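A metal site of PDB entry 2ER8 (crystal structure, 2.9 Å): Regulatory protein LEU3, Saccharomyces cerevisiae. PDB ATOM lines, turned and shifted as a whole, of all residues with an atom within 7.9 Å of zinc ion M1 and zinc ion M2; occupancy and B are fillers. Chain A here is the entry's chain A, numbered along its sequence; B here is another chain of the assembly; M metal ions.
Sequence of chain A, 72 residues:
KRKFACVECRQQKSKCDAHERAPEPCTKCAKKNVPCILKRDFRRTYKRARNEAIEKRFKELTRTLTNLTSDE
The backbone carbonyl oxygen of Cys 29 is in hydrogen-bond range of the backbone NH of Val 34, 2.9 Å away.
The side-chain sulfur (SG) of Cys 6 sits close to the backbone NH (N) of Glu 8 of chain A (3.7 Å).
The backbone NH (N) of Ser 14 is in hydrogen-bond range of the backbone carbonyl oxygen (O) of Cys 9.
The side-chain sulfur (SG) of Cys 16 sits close to the backbone NH (N) of Ala 18, at 3.2 Å.
N of Cys 16 sits at hydrogen-bond distance from OP2 of DC 8 of chain B, at 3.1 Å.
Of the 26 residues printed, 4 come within 4 Å of zinc ion M1.
The nearest printed residue that does not touch zinc ion M1 is Ala 18 (4.4 Å).
Four residues have an atom within 4 Å of zinc ion M2: Cys 6, Cys 26, Cys 29 and Cys 36.
Zinc ion M1 is bound by the side-chain sulfur of Cys 26 (2.4 Å), the side-chain sulfur of Cys 9 (2.4 Å), the side-chain sulfur of Cys 16 (2.5 Å) and the side-chain sulfur of Cys 6 (2.6 Å).
Zinc ion M2 is bound by SG of Cys 29 (2.1 Å), SG of Cys 36 (2.3 Å), SG of Cys 26 (2.4 Å) and SG of Cys 6 (2.4 Å).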
ATOM      1  N   PHE A   4      -0.637  31.625   6.554  1.00  0.00           N
ATOM      2  CA  PHE A   4      -1.081  32.144   5.255  1.00  0.00           C
ATOM      3  C   PHE A   4      -2.476  31.629   4.837  1.00  0.00           C
ATOM      4  O   PHE A   4      -2.889  30.554   5.268  1.00  0.00           O
ATOM      5  CB  PHE A   4      -0.014  31.862   4.169  1.00  0.00           C
ATOM      6  CG  PHE A   4       0.114  30.403   3.781  1.00  0.00           C
ATOM      7  CD1 PHE A   4       0.335  30.049   2.437  1.00  0.00           C
ATOM      8  CD2 PHE A   4       0.047  29.395   4.744  1.00  0.00           C
ATOM      9  CE1 PHE A   4       0.475  28.726   2.061  1.00  0.00           C
ATOM     10  CE2 PHE A   4       0.188  28.063   4.382  1.00  0.00           C
ATOM     11  CZ  PHE A   4       0.409  27.719   3.024  1.00  0.00           C
ATOM     12  N   ALA A   5      -3.210  32.399   4.025  1.00  0.00           N
ATOM     13  CA  ALA A   5      -4.539  32.013   3.543  1.00  0.00           C
ATOM     14  C   ALA A   5      -4.442  31.125   2.287  1.00  0.00           C
ATOM     15  O   ALA A   5      -3.451  31.135   1.526  1.00  0.00           O
ATOM     16  CB  ALA A   5      -5.334  33.241   3.244  1.00  0.00           C
ATOM     17  N   CYS A   6      -5.487  30.325   2.059  1.00  0.00           N
ATOM     18  CA  CYS A   6      -5.491  29.416   0.944  1.00  0.00           C
ATOM     19  C   CYS A   6      -5.725  30.191  -0.328  1.00  0.00           C
ATOM     20  O   CYS A   6      -6.287  31.279  -0.320  1.00  0.00           O
ATOM     21  CB  CYS A   6      -6.601  28.394   1.097  1.00  0.00           C
ATOM     22  SG  CYS A   6      -8.136  29.065   0.611  1.00  0.00           S
ATOM     23  N   VAL A   7      -5.265  29.602  -1.426  1.00  0.00           N
ATOM     24  CA  VAL A   7      -5.390  30.203  -2.730  1.00  0.00           C
ATOM     25  C   VAL A   7      -6.683  30.929  -2.963  1.00  0.00           C
ATOM     26  O   VAL A   7      -6.687  32.112  -3.181  1.00  0.00           O
ATOM     27  CB  VAL A   7      -5.280  29.149  -3.791  1.00  0.00           C
ATOM     28  CG1 VAL A   7      -5.344  29.763  -5.150  1.00  0.00           C
ATOM     29  CG2 VAL A   7      -3.993  28.389  -3.586  1.00  0.00           C
ATOM     30  N   GLU A   8      -7.785  30.191  -2.937  1.00  0.00           N
ATOM     31  CA  GLU A   8      -9.094  30.771  -3.180  1.00  0.00           C
ATOM     32  C   GLU A   8      -9.396  31.954  -2.298  1.00  0.00           C
ATOM     33  O   GLU A   8      -9.883  32.968  -2.786  1.00  0.00           O
ATOM     34  CB  GLU A   8     -10.191  29.725  -3.002  1.00  0.00           C
ATOM     35  CG  GLU A   8     -11.546  30.189  -3.475  1.00  0.00           C
ATOM     36  CD  GLU A   8     -11.495  30.865  -4.854  1.00  0.00           C
ATOM     37  OE1 GLU A   8     -10.674  30.446  -5.698  1.00  0.00           O
ATOM     38  OE2 GLU A   8     -12.282  31.815  -5.112  1.00  0.00           O
ATOM     39  N   CYS A   9      -9.116  31.863  -1.002  1.00  0.00           N
ATOM     40  CA  CYS A   9      -9.378  33.007  -0.147  1.00  0.00           C
ATOM     41  C   CYS A   9      -8.526  34.190  -0.509  1.00  0.00           C
ATOM     42  O   CYS A   9      -8.985  35.319  -0.452  1.00  0.00           O
ATOM     43  CB  CYS A   9      -9.189  32.621   1.287  1.00  0.00           C
ATOM     44  SG  CYS A   9     -10.574  31.609   1.647  1.00  0.00           S
ATOM     45  N   ARG A  10      -7.287  33.939  -0.932  1.00  0.00           N
ATOM     46  CA  ARG A  10      -6.409  35.026  -1.391  1.00  0.00           C
ATOM     47  C   ARG A  10      -6.939  35.690  -2.649  1.00  0.00           C
ATOM     48  O   ARG A  10      -6.907  36.900  -2.789  1.00  0.00           O
ATOM     49  CB  ARG A  10      -5.017  34.525  -1.697  1.00  0.00           C
ATOM     50  CG  ARG A  10      -4.167  34.400  -0.490  1.00  0.00           C
ATOM     51  CD  ARG A  10      -2.760  34.143  -0.874  1.00  0.00           C
ATOM     52  NE  ARG A  10      -1.929  34.195   0.317  1.00  0.00           N
ATOM     53  CZ  ARG A  10      -0.642  33.875   0.309  1.00  0.00           C
ATOM     54  NH1 ARG A  10      -0.076  33.489  -0.820  1.00  0.00           N
ATOM     55  NH2 ARG A  10       0.058  33.928   1.435  1.00  0.00           N
ATOM     56  N   SER A  14     -10.782  37.082   0.893  1.00  0.00           N
ATOM     57  CA  SER A  14     -11.733  36.725   1.951  1.00  0.00           C
ATOM     58  C   SER A  14     -11.049  36.074   3.177  1.00  0.00           C
ATOM     59  O   SER A  14      -9.946  35.467   3.061  1.00  0.00           O
ATOM     60  CB  SER A  14     -12.796  35.764   1.381  1.00  0.00           C
ATOM     61  OG  SER A  14     -12.235  34.511   1.041  1.00  0.00           O
ATOM     62  N   LYS A  15     -11.687  36.210   4.335  1.00  0.00           N
ATOM     63  CA  LYS A  15     -11.140  35.609   5.535  1.00  0.00           C
ATOM     64  C   LYS A  15     -11.054  34.080   5.345  1.00  0.00           C
ATOM     65  O   LYS A  15     -12.039  33.397   5.018  1.00  0.00           O
ATOM     66  CB  LYS A  15     -11.996  35.910   6.744  1.00  0.00           C
ATOM     67  CG  LYS A  15     -11.379  35.363   7.997  1.00  0.00           C
ATOM     68  CD  LYS A  15     -12.361  35.380   9.125  1.00  0.00           C
ATOM     69  CE  LYS A  15     -11.781  34.633  10.293  1.00  0.00           C
ATOM     70  NZ  LYS A  15     -10.396  35.121  10.530  1.00  0.00           N
ATOM     71  N   CYS A  16      -9.835  33.571   5.533  1.00  0.00           N
ATOM     72  CA  CYS A  16      -9.571  32.151   5.385  1.00  0.00           C
ATOM     73  C   CYS A  16      -9.173  31.557   6.719  1.00  0.00           C
ATOM     74  O   CYS A  16      -8.319  32.095   7.417  1.00  0.00           O
ATOM     75  CB  CYS A  16      -8.467  31.927   4.369  1.00  0.00           C
ATOM     76  SG  CYS A  16      -7.716  30.336   4.444  1.00  0.00           S
ATOM     77  N   ASP A  17      -9.796  30.456   7.065  1.00  0.00           N
ATOM     78  CA  ASP A  17      -9.503  29.773   8.305  1.00  0.00           C
ATOM     79  C   ASP A  17      -8.878  28.401   7.997  1.00  0.00           C
ATOM     80  O   ASP A  17      -8.807  27.558   8.875  1.00  0.00           O
ATOM     81  CB  ASP A  17     -10.790  29.579   9.102  1.00  0.00           C
ATOM     82  CG  ASP A  17     -11.757  28.593   8.437  1.00  0.00           C
ATOM     83  OD1 ASP A  17     -11.591  28.275   7.228  1.00  0.00           O
ATOM     84  OD2 ASP A  17     -12.698  28.137   9.138  1.00  0.00           O
ATOM     85  N   ALA A  18      -8.448  28.185   6.762  1.00  0.00           N
ATOM     86  CA  ALA A  18      -7.860  26.904   6.363  1.00  0.00           C
ATOM     87  C   ALA A  18      -7.090  26.262   7.489  1.00  0.00           C
ATOM     88  O   ALA A  18      -7.275  25.069   7.734  1.00  0.00           O
ATOM     89  CB  ALA A  18      -6.951  27.089   5.162  1.00  0.00           C
ATOM     90  N   HIS A  19      -6.250  27.029   8.170  1.00  0.00           N
ATOM     91  CA  HIS A  19      -5.434  26.506   9.260  1.00  0.00           C
ATOM     92  C   HIS A  19      -6.262  25.928  10.400  1.00  0.00           C
ATOM     93  O   HIS A  19      -6.217  24.714  10.672  1.00  0.00           O
ATOM     94  CB  HIS A  19      -4.509  27.592   9.806  1.00  0.00           C
ATOM     95  CG  HIS A  19      -3.560  28.127   8.785  1.00  0.00           C
ATOM     96  ND1 HIS A  19      -2.508  27.377   8.270  1.00  0.00           N
ATOM     97  CD2 HIS A  19      -3.490  29.333   8.169  1.00  0.00           C
ATOM     98  CE1 HIS A  19      -1.848  28.091   7.388  1.00  0.00           C
ATOM     99  NE2 HIS A  19      -2.417  29.289   7.302  1.00  0.00           N
ATOM    100  N   GLU A  24      -9.722  19.352   6.779  1.00  0.00           N
ATOM    101  CA  GLU A  24     -10.943  19.836   6.170  1.00  0.00           C
ATOM    102  C   GLU A  24     -10.710  21.204   5.528  1.00  0.00           C
ATOM    103  O   GLU A  24     -10.180  22.116   6.161  1.00  0.00           O
ATOM    104  CB  GLU A  24     -12.043  19.923   7.230  1.00  0.00           C
ATOM    105  CG  GLU A  24     -12.288  18.614   7.964  1.00  0.00           C
ATOM    106  CD  GLU A  24     -12.531  17.449   7.017  1.00  0.00           C
ATOM    107  OE1 GLU A  24     -13.510  17.509   6.239  1.00  0.00           O
ATOM    108  OE2 GLU A  24     -11.739  16.480   7.029  1.00  0.00           O
ATOM    109  N   PRO A  25     -11.095  21.357   4.241  1.00  0.00           N
ATOM    110  CA  PRO A  25     -10.940  22.589   3.473  1.00  0.00           C
ATOM    111  C   PRO A  25     -11.426  23.799   4.256  1.00  0.00           C
ATOM    112  O   PRO A  25     -12.296  23.668   5.113  1.00  0.00           O
ATOM    113  CB  PRO A  25     -11.784  22.341   2.220  1.00  0.00           C
ATOM    114  CG  PRO A  25     -11.547  20.888   1.976  1.00  0.00           C
ATOM    115  CD  PRO A  25     -11.697  20.308   3.393  1.00  0.00           C
ATOM    116  N   CYS A  26     -10.881  24.979   3.962  1.00  0.00           N
ATOM    117  CA  CYS A  26     -11.285  26.183   4.683  1.00  0.00           C
ATOM    118  C   CYS A  26     -12.759  26.373   4.430  1.00  0.00           C
ATOM    119  O   CYS A  26     -13.289  25.985   3.385  1.00  0.00           O
ATOM    120  CB  CYS A  26     -10.505  27.415   4.223  1.00  0.00           C
ATOM    121  SG  CYS A  26     -11.032  28.050   2.618  1.00  0.00           S
ATOM    122  N   THR A  27     -13.421  26.943   5.433  1.00  0.00           N
ATOM    123  CA  THR A  27     -14.848  27.214   5.387  1.00  0.00           C
ATOM    124  C   THR A  27     -15.264  27.691   4.000  1.00  0.00           C
ATOM    125  O   THR A  27     -16.024  27.019   3.295  1.00  0.00           O
ATOM    126  CB  THR A  27     -15.225  28.292   6.424  1.00  0.00           C
ATOM    127  OG1 THR A  27     -14.833  27.870   7.738  1.00  0.00           O
ATOM    128  CG2 THR A  27     -16.703  28.520   6.401  1.00  0.00           C
ATOM    129  N   LYS A  28     -14.742  28.858   3.617  1.00  0.00           N
ATOM    130  CA  LYS A  28     -15.028  29.480   2.331  1.00  0.00           C
ATOM    131  C   LYS A  28     -14.911  28.528   1.151  1.00  0.00           C
ATOM    132  O   LYS A  28     -15.798  28.501   0.294  1.00  0.00           O
ATOM    133  CB  LYS A  28     -14.095  30.671   2.121  1.00  0.00           C
ATOM    134  CG  LYS A  28     -14.416  31.911   2.965  1.00  0.00           C
ATOM    135  CD  LYS A  28     -15.609  32.626   2.392  1.00  0.00           C
ATOM    136  CE  LYS A  28     -15.885  33.944   3.038  1.00  0.00           C
ATOM    137  NZ  LYS A  28     -17.083  34.609   2.386  1.00  0.00           N
ATOM    138  N   CYS A  29     -13.835  27.746   1.108  1.00  0.00           N
ATOM    139  CA  CYS A  29     -13.599  26.790   0.010  1.00  0.00           C
ATOM    140  C   CYS A  29     -14.620  25.649  -0.012  1.00  0.00           C
ATOM    141  O   CYS A  29     -15.030  25.171  -1.063  1.00  0.00           O
ATOM    142  CB  CYS A  29     -12.183  26.201   0.066  1.00  0.00           C
ATOM    143  SG  CYS A  29     -10.917  27.248  -0.687  1.00  0.00           S
ATOM    144  N   ALA A  30     -15.003  25.208   1.179  1.00  0.00           N
ATOM    145  CA  ALA A  30     -15.994  24.169   1.303  1.00  0.00           C
ATOM    146  C   ALA A  30     -17.342  24.675   0.740  1.00  0.00           C
ATOM    147  O   ALA A  30     -17.933  24.056  -0.162  1.00  0.00           O
ATOM    148  CB  ALA A  30     -16.140  23.797   2.763  1.00  0.00           C
ATOM    149  N   VAL A  34     -15.074  23.753  -3.592  1.00  0.00           N
ATOM    150  CA  VAL A  34     -13.850  23.779  -4.370  1.00  0.00           C
ATOM    151  C   VAL A  34     -12.681  23.387  -3.503  1.00  0.00           C
ATOM    152  O   VAL A  34     -12.705  23.512  -2.270  1.00  0.00           O
ATOM    153  CB  VAL A  34     -13.570  25.176  -4.975  1.00  0.00           C
ATOM    154  CG1 VAL A  34     -14.631  25.532  -5.986  1.00  0.00           C
ATOM    155  CG2 VAL A  34     -13.529  26.220  -3.872  1.00  0.00           C
ATOM    156  N   PRO A  35     -11.619  22.887  -4.145  1.00  0.00           N
ATOM    157  CA  PRO A  35     -10.398  22.453  -3.470  1.00  0.00           C
ATOM    158  C   PRO A  35      -9.710  23.579  -2.707  1.00  0.00           C
ATOM    159  O   PRO A  35      -9.406  24.637  -3.268  1.00  0.00           O
ATOM    160  CB  PRO A  35      -9.549  21.924  -4.625  1.00  0.00           C
ATOM    161  CG  PRO A  35     -10.565  21.440  -5.592  1.00  0.00           C
ATOM    162  CD  PRO A  35     -11.586  22.542  -5.573  1.00  0.00           C
ATOM    163  N   CYS A  36      -9.446  23.343  -1.421  1.00  0.00           N
ATOM    164  CA  CYS A  36      -8.768  24.346  -0.626  1.00  0.00           C
ATOM    165  C   CYS A  36      -7.265  24.115  -0.728  1.00  0.00           C
ATOM    166  O   CYS A  36      -6.681  23.379   0.070  1.00  0.00           O
ATOM    167  CB  CYS A  36      -9.220  24.240   0.823  1.00  0.00           C
ATOM    168  SG  CYS A  36      -8.488  25.437   1.898  1.00  0.00           S
ATOM    169  N   ILE A  37      -6.633  24.754  -1.705  1.00  0.00           N
ATOM    170  CA  ILE A  37      -5.211  24.576  -1.909  1.00  0.00           C
ATOM    171  C   ILE A  37      -4.376  25.654  -1.256  1.00  0.00           C
ATOM    172  O   ILE A  37      -4.787  26.805  -1.227  1.00  0.00           O
ATOM    173  CB  ILE A  37      -4.915  24.565  -3.399  1.00  0.00           C
ATOM    174  CG1 ILE A  37      -5.731  23.457  -4.058  1.00  0.00           C
ATOM    175  CG2 ILE A  37      -3.445  24.344  -3.625  1.00  0.00           C
ATOM    176  CD1 ILE A  37      -5.559  23.321  -5.549  1.00  0.00           C
ATOM    177  N   LEU A  38      -3.212  25.292  -0.711  1.00  0.00           N
ATOM    178  CA  LEU A  38      -2.307  26.285  -0.101  1.00  0.00           C
ATOM    179  C   LEU A  38      -1.001  26.450  -0.904  1.00  0.00           C
ATOM    180  O   LEU A  38      -0.341  25.461  -1.229  1.00  0.00           O
ATOM    181  CB  LEU A  38      -1.950  25.900   1.334  1.00  0.00           C
ATOM    182  CG  LEU A  38      -3.064  25.326   2.204  1.00  0.00           C
ATOM    183  CD1 LEU A  38      -2.780  25.628   3.662  1.00  0.00           C
ATOM    184  CD2 LEU A  38      -4.390  25.920   1.834  1.00  0.00           C
ATOM    185  P    DC B   8      -7.497  36.202   7.592  1.00  0.00           P
ATOM    186  OP1  DC B   8      -7.780  35.311   8.760  1.00  0.00           O
ATOM    187  OP2  DC B   8      -7.681  35.727   6.178  1.00  0.00           O
ATOM    188  O5'  DC B   8      -8.387  37.491   7.794  1.00  0.00           O
ATOM    189  C5'  DC B   8      -7.887  38.698   7.308  1.00  0.00           C
ATOM    190  C4'  DC B   8      -8.928  39.765   7.421  1.00  0.00           C
ATOM    191  O4'  DC B   8      -8.541  40.832   6.540  1.00  0.00           O
ATOM    192  C3'  DC B   8     -10.302  39.310   6.938  1.00  0.00           C
ATOM    193  O3'  DC B   8     -11.239  40.047   7.721  1.00  0.00           O
ATOM    194  C2'  DC B   8     -10.238  39.624   5.443  1.00  0.00           C
ATOM    195  C1'  DC B   8      -9.371  40.881   5.401  1.00  0.00           C
ATOM    196  N1   DC B   8      -8.493  41.049   4.224  1.00  0.00           N
ATOM    197  C2   DC B   8      -8.191  42.331   3.826  1.00  0.00           C
ATOM    198  O2   DC B   8      -8.616  43.271   4.523  1.00  0.00           O
ATOM    199  N3   DC B   8      -7.438  42.532   2.716  1.00  0.00           N
ATOM    200  C4   DC B   8      -6.986  41.485   2.018  1.00  0.00           C
ATOM    201  N4   DC B   8      -6.262  41.742   0.924  1.00  0.00           N
ATOM    202  C5   DC B   8      -7.253  40.147   2.427  1.00  0.00           C
ATOM    203  C6   DC B   8      -8.015  39.969   3.525  1.00  0.00           C
HETATM  204 ZN    ZN M   1      -9.416  29.780   2.722  1.00  0.00          ZN
HETATM  205 ZN    ZN M   2      -9.582  27.203   0.966  1.00  0.00          ZN
